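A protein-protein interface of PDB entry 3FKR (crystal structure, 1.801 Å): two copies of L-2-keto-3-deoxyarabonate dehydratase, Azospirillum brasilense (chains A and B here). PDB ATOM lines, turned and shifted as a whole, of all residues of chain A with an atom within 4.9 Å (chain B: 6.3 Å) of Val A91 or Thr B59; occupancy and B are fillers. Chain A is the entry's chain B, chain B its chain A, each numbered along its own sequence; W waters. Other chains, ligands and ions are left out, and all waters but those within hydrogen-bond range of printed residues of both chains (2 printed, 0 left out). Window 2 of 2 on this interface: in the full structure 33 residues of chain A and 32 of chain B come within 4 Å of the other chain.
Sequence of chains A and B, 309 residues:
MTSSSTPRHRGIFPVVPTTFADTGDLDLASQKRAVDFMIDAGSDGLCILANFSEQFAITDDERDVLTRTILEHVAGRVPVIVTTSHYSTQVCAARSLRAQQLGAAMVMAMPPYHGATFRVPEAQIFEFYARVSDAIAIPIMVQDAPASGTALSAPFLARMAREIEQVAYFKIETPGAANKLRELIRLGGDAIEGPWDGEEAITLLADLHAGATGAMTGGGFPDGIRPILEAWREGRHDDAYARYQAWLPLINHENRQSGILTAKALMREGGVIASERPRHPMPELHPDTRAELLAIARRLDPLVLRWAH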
ATOM      1  N   ASP A  60      11.039  19.082  22.019  1.00  0.00           N
ATOM      2  CA  ASP A  60       9.934  18.770  21.072  1.00  0.00           C
ATOM      3  C   ASP A  60       9.672  19.901  20.091  1.00  0.00           C
ATOM      4  O   ASP A  60       9.334  19.667  18.917  1.00  0.00           O
ATOM      5  CB  ASP A  60       8.593  18.612  21.851  1.00  0.00           C
ATOM      6  CG  ASP A  60       8.541  17.304  22.737  1.00  0.00           C
ATOM      7  OD1 ASP A  60       7.583  17.209  23.522  1.00  0.00           O
ATOM      8  OD2 ASP A  60       9.402  16.397  22.664  1.00  0.00           O
ATOM      9  N   HIS A  86       8.832   7.612  20.516  1.00  0.00           N
ATOM     10  CA  HIS A  86       8.476   8.156  21.844  1.00  0.00           C
ATOM     11  C   HIS A  86       7.921   6.953  22.634  1.00  0.00           C
ATOM     12  O   HIS A  86       7.445   5.971  22.039  1.00  0.00           O
ATOM     13  CB  HIS A  86       7.406   9.249  21.717  1.00  0.00           C
ATOM     14  CG  HIS A  86       7.175   9.977  23.004  1.00  0.00           C
ATOM     15  ND1 HIS A  86       7.813  11.157  23.329  1.00  0.00           N
ATOM     16  CD2 HIS A  86       6.380   9.677  24.053  1.00  0.00           C
ATOM     17  CE1 HIS A  86       7.442  11.543  24.541  1.00  0.00           C
ATOM     18  NE2 HIS A  86       6.563  10.665  24.993  1.00  0.00           N
ATOM     19  N   SER A  88       5.305   6.896  24.627  1.00  0.00           N
ATOM     20  CA  SER A  88       3.824   6.875  24.537  1.00  0.00           C
ATOM     21  C   SER A  88       3.373   6.485  23.150  1.00  0.00           C
ATOM     22  O   SER A  88       3.796   7.142  22.171  1.00  0.00           O
ATOM     23  CB  SER A  88       3.227   8.229  24.895  1.00  0.00           C
ATOM     24  OG  SER A  88       1.867   8.296  24.454  1.00  0.00           O
ATOM     25  N   THR A  89       2.526   5.457  23.037  1.00  0.00           N
ATOM     26  CA  THR A  89       1.935   5.068  21.754  1.00  0.00           C
ATOM     27  C   THR A  89       1.197   6.244  21.152  1.00  0.00           C
ATOM     28  O   THR A  89       1.330   6.515  19.956  1.00  0.00           O
ATOM     29  CB  THR A  89       0.914   3.952  21.906  1.00  0.00           C
ATOM     30  OG1 THR A  89       1.553   2.849  22.604  1.00  0.00           O
ATOM     31  CG2 THR A  89       0.340   3.453  20.544  1.00  0.00           C
ATOM     32  N   GLN A  90       0.353   6.912  21.959  1.00  0.00           N
ATOM     33  CA  GLN A  90      -0.444   8.012  21.431  1.00  0.00           C
ATOM     34  C   GLN A  90       0.434   9.183  20.936  1.00  0.00           C
ATOM     35  O   GLN A  90       0.155   9.784  19.871  1.00  0.00           O
ATOM     36  CB  GLN A  90      -1.483   8.467  22.503  1.00  0.00           C
ATOM     37  CG  GLN A  90      -2.536   7.318  22.751  1.00  0.00           C
ATOM     38  CD  GLN A  90      -3.245   7.525  24.082  1.00  0.00           C
ATOM     39  OE1 GLN A  90      -2.627   7.422  25.131  1.00  0.00           O
ATOM     40  NE2 GLN A  90      -4.539   7.878  24.030  1.00  0.00           N
ATOM     41  N   VAL A  91       1.486   9.492  21.680  1.00  0.00           N
ATOM     42  CA  VAL A  91       2.399  10.543  21.255  1.00  0.00           C
ATOM     43  C   VAL A  91       3.095  10.143  19.962  1.00  0.00           C
ATOM     44  O   VAL A  91       3.252  10.958  19.071  1.00  0.00           O
ATOM     45  CB  VAL A  91       3.481  10.863  22.300  1.00  0.00           C
ATOM     46  CG1 VAL A  91       4.505  11.928  21.758  1.00  0.00           C
ATOM     47  CG2 VAL A  91       2.859  11.338  23.640  1.00  0.00           C
ATOM     48  N   CYS A  92       3.549   8.885  19.888  1.00  0.00           N
ATOM     49  CA  CYS A  92       4.257   8.467  18.681  1.00  0.00           C
ATOM     50  C   CYS A  92       3.309   8.484  17.504  1.00  0.00           C
ATOM     51  O   CYS A  92       3.674   8.912  16.393  1.00  0.00           O
ATOM     52  CB  CYS A  92       4.907   7.084  18.842  1.00  0.00           C
ATOM     53  SG  CYS A  92       5.818   6.474  17.329  1.00  0.00           S
ATOM     54  N   ALA A  93       2.092   7.977  17.722  1.00  0.00           N
ATOM     55  CA  ALA A  93       1.120   7.969  16.661  1.00  0.00           C
ATOM     56  C   ALA A  93       0.870   9.384  16.154  1.00  0.00           C
ATOM     57  O   ALA A  93       0.749   9.558  14.940  1.00  0.00           O
ATOM     58  CB  ALA A  93      -0.197   7.340  17.106  1.00  0.00           C
ATOM     59  N   ALA A  94       0.795  10.363  17.083  1.00  0.00           N
ATOM     60  CA  ALA A  94       0.488  11.752  16.717  1.00  0.00           C
ATOM     61  C   ALA A  94       1.650  12.346  15.942  1.00  0.00           C
ATOM     62  O   ALA A  94       1.430  13.072  14.957  1.00  0.00           O
ATOM     63  CB  ALA A  94       0.139  12.661  17.964  1.00  0.00           C
ATOM     64  N   ARG A  95       2.862  12.065  16.379  1.00  0.00           N
ATOM     65  CA  ARG A  95       4.057  12.540  15.650  1.00  0.00           C
ATOM     66  C   ARG A  95       4.148  11.963  14.256  1.00  0.00           C
ATOM     67  O   ARG A  95       4.488  12.670  13.291  1.00  0.00           O
ATOM     68  CB  ARG A  95       5.322  12.284  16.453  1.00  0.00           C
ATOM     69  CG  ARG A  95       5.301  13.120  17.684  1.00  0.00           C
ATOM     70  CD  ARG A  95       6.593  13.067  18.441  1.00  0.00           C
ATOM     71  NE  ARG A  95       6.435  13.804  19.683  1.00  0.00           N
ATOM     72  CZ  ARG A  95       7.397  14.029  20.575  1.00  0.00           C
ATOM     73  NH1 ARG A  95       8.631  13.565  20.400  1.00  0.00           N
ATOM     74  NH2 ARG A  95       7.097  14.705  21.661  1.00  0.00           N
ATOM     75  N   GLN B  55       7.062  10.412  33.893  1.00  0.00           N
ATOM     76  CA  GLN B  55       7.469  11.571  33.074  1.00  0.00           C
ATOM     77  C   GLN B  55       7.916  11.196  31.641  1.00  0.00           C
ATOM     78  O   GLN B  55       7.697  11.960  30.722  1.00  0.00           O
ATOM     79  CB  GLN B  55       8.508  12.381  33.812  1.00  0.00           C
ATOM     80  CG  GLN B  55       9.813  11.742  33.830  1.00  0.00           C
ATOM     81  CD  GLN B  55      10.557  12.000  32.507  1.00  0.00           C
ATOM     82  OE1 GLN B  55      10.282  12.958  31.763  1.00  0.00           O
ATOM     83  NE2 GLN B  55      11.468  11.148  32.214  1.00  0.00           N
ATOM     84  N   ALA B  57       6.422   9.205  29.668  1.00  0.00           N
ATOM     85  CA  ALA B  57       5.266   9.040  28.779  1.00  0.00           C
ATOM     86  C   ALA B  57       4.580  10.356  28.381  1.00  0.00           C
ATOM     87  O   ALA B  57       3.514  10.324  27.719  1.00  0.00           O
ATOM     88  CB  ALA B  57       4.210   8.060  29.425  1.00  0.00           C
ATOM     89  N   ILE B  58       5.114  11.502  28.810  1.00  0.00           N
ATOM     90  CA  ILE B  58       4.464  12.734  28.472  1.00  0.00           C
ATOM     91  C   ILE B  58       5.334  13.616  27.532  1.00  0.00           C
ATOM     92  O   ILE B  58       6.508  13.299  27.273  1.00  0.00           O
ATOM     93  CB  ILE B  58       4.026  13.532  29.729  1.00  0.00           C
ATOM     94  CG1 ILE B  58       5.242  13.992  30.532  1.00  0.00           C
ATOM     95  CG2 ILE B  58       2.961  12.698  30.605  1.00  0.00           C
ATOM     96  CD1 ILE B  58       4.856  14.939  31.713  1.00  0.00           C
ATOM     97  N   THR B  59       4.743  14.685  27.030  1.00  0.00           N
ATOM     98  CA  THR B  59       5.444  15.584  26.098  1.00  0.00           C
ATOM     99  C   THR B  59       6.055  16.759  26.849  1.00  0.00           C
ATOM    100  O   THR B  59       5.772  16.994  28.037  1.00  0.00           O
ATOM    101  CB  THR B  59       4.514  16.098  25.062  1.00  0.00           C
ATOM    102  OG1 THR B  59       3.548  16.973  25.666  1.00  0.00           O
ATOM    103  CG2 THR B  59       3.795  14.949  24.375  1.00  0.00           C
ATOM    104  N   ASP B  60       6.885  17.555  26.180  1.00  0.00           N
ATOM    105  CA  ASP B  60       7.386  18.741  26.887  1.00  0.00           C
ATOM    106  C   ASP B  60       6.250  19.720  27.304  1.00  0.00           C
ATOM    107  O   ASP B  60       6.311  20.393  28.345  1.00  0.00           O
ATOM    108  CB  ASP B  60       8.334  19.543  25.987  1.00  0.00           C
ATOM    109  CG  ASP B  60       9.664  18.817  25.677  1.00  0.00           C
ATOM    110  OD1 ASP B  60      10.398  19.305  24.787  1.00  0.00           O
ATOM    111  OD2 ASP B  60       9.996  17.835  26.331  1.00  0.00           O
ATOM    112  N   ASP B  61       5.274  19.866  26.417  1.00  0.00           N
ATOM    113  CA  ASP B  61       4.157  20.801  26.605  1.00  0.00           C
ATOM    114  C   ASP B  61       3.380  20.304  27.830  1.00  0.00           C
ATOM    115  O   ASP B  61       3.006  21.092  28.723  1.00  0.00           O
ATOM    116  CB  ASP B  61       3.223  20.708  25.388  1.00  0.00           C
ATOM    117  CG  ASP B  61       3.650  21.584  24.206  1.00  0.00           C
ATOM    118  OD1 ASP B  61       4.572  22.423  24.347  1.00  0.00           O
ATOM    119  OD2 ASP B  61       3.047  21.384  23.119  1.00  0.00           O
ATOM    120  N   GLU B  62       3.179  18.978  27.902  1.00  0.00           N
ATOM    121  CA  GLU B  62       2.472  18.420  29.125  1.00  0.00           C
ATOM    122  C   GLU B  62       3.256  18.652  30.407  1.00  0.00           C
ATOM    123  O   GLU B  62       2.735  18.996  31.463  1.00  0.00           O
ATOM    124  CB  GLU B  62       2.082  16.975  28.873  1.00  0.00           C
ATOM    125  CG  GLU B  62       1.058  16.852  27.743  1.00  0.00           C
ATOM    126  CD  GLU B  62       0.837  15.431  27.299  1.00  0.00           C
ATOM    127  OE1 GLU B  62       1.768  14.623  27.475  1.00  0.00           O
ATOM    128  OE2 GLU B  62      -0.247  15.100  26.794  1.00  0.00           O
ATOM    129  N   ARG B  63       4.566  18.495  30.330  1.00  0.00           N
ATOM    130  CA  ARG B  63       5.450  18.739  31.456  1.00  0.00           C
ATOM    131  C   ARG B  63       5.289  20.161  31.995  1.00  0.00           C
ATOM    132  O   ARG B  63       5.260  20.394  33.219  1.00  0.00           O
ATOM    133  CB  ARG B  63       6.881  18.495  30.939  1.00  0.00           C
ATOM    134  CG  ARG B  63       8.055  18.409  31.920  1.00  0.00           C
ATOM    135  CD  ARG B  63       9.364  17.975  31.133  1.00  0.00           C
ATOM    136  NE  ARG B  63       9.018  16.858  30.260  1.00  0.00           N
ATOM    137  CZ  ARG B  63       9.188  15.576  30.579  1.00  0.00           C
ATOM    138  NH1 ARG B  63       9.776  15.260  31.716  1.00  0.00           N
ATOM    139  NH2 ARG B  63       8.788  14.616  29.753  1.00  0.00           N
ATOM    140  N   ASP B  64       5.233  21.128  31.077  1.00  0.00           N
ATOM    141  CA  ASP B  64       5.104  22.524  31.479  1.00  0.00           C
ATOM    142  C   ASP B  64       3.744  22.782  32.098  1.00  0.00           C
ATOM    143  O   ASP B  64       3.646  23.460  33.134  1.00  0.00           O
ATOM    144  CB  ASP B  64       5.271  23.434  30.265  1.00  0.00           C
ATOM    145  CG  ASP B  64       5.381  24.884  30.703  1.00  0.00           C
ATOM    146  OD1 ASP B  64       6.434  25.236  31.290  1.00  0.00           O
ATOM    147  OD2 ASP B  64       4.398  25.621  30.566  1.00  0.00           O
ATOM    148  N   ARG B 279      -0.243   5.480  30.643  1.00  0.00           N
ATOM    149  CA  ARG B 279      -0.460   5.553  29.173  1.00  0.00           C
ATOM    150  C   ARG B 279       0.074   4.298  28.456  1.00  0.00           C
ATOM    151  O   ARG B 279       1.178   3.827  28.769  1.00  0.00           O
ATOM    152  CB  ARG B 279       0.274   6.805  28.611  1.00  0.00           C
ATOM    153  CG  ARG B 279      -0.528   8.079  28.789  1.00  0.00           C
ATOM    154  CD  ARG B 279       0.237   9.284  28.164  1.00  0.00           C
ATOM    155  NE  ARG B 279      -0.656  10.422  28.146  1.00  0.00           N
ATOM    156  CZ  ARG B 279      -0.300  11.654  27.808  1.00  0.00           C
ATOM    157  NH1 ARG B 279       0.943  11.892  27.404  1.00  0.00           N
ATOM    158  NH2 ARG B 279      -1.212  12.631  27.824  1.00  0.00           N
HETATM  159  O   HOH W   1       5.514  19.126  23.439  1.00  0.00           O
HETATM  160  O   HOH W   2       9.456  21.794  23.490  1.00  0.00           O
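NE2 of His A86 sits close to O of Ile B58, 3.5 Å away. OD1 of Asp A60 is in hydrogen-bond range of N of Asp B60 (2.8 Å).
The side-chain carboxylate of Glu B62 lies within hydrogen-bond range of the backbone NH of Thr B59, at 3.0 Å. OD2 of Asp A60 is in salt-bridge range of NH2 of Arg A95. OG of Ser A88 sits at hydrogen-bond distance from N of Gln A90, at 3.2 Å. N of Val A91 is in hydrogen-bond range of OG of Ser A88 (3.0 Å). The side-chain hydroxyl (OG1) of Thr B59 lies close to the backbone NH (N) of Asp B61 (3.5 Å). The backbone carbonyl oxygen (O) of Ala B57 lies within hydrogen-bond range of the guanidinium group (NH1) of Arg B279, 3.0 Å away.
Thr B59 touches Asp A60. Ala B57 touches His A86 (C to NE2, 3.9 Å). CB of Ser A88 touches O of Ala B57 (3.5 Å). Val A91 touches Thr B59.
Printed residues of chain B within 4 Å of His A86: Ala B57 (3.9 Å) and Ile B58 (3.4 Å). Thr A89 touches none of the printed residues of chain B. Val A91 touches just one residue of chain B: Thr B59. Of the printed residues of chain A, Ile B58 touches His A86 (3.4 Å). Thr B59 touches just these residues of chain A: Asp A60 and Val A91. Glu B62 touches none of the printed residues of chain A. The nearest printed residue of chain B that does not touch Val A91 is Ala B57 (4.3 Å). The nearest printed residue of chain A that does not touch Thr B59 is Arg A95 (4.3 Å). The nearest printed residue of chain B that does not touch His A86 is Thr B59 (4.8 Å).
Along chain B the printed residues that touch a printed residue of chain A span positions 57 to 60. Hydrophobic or aromatic side chains of chain A within 4 Å of the printed part of chain B: His A86 and Val A91.
Asp B60 touches its own counterpart, Asp A60. Position printed for both chains: 60. Of the 6 pairs that touch across the chains among the printed residues, 1 has its exchanged pair printed and touching as well.
Water W1 lies within hydrogen-bond range of OD1 of Asp A60 (2.8 Å), N of Asp B61 (3.1 Å) and N of Asp B60 (3.4 Å). Water W2 lies within hydrogen-bond range of the side-chain carboxylate of Asp B60 and the backbone NH of Asp A60.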
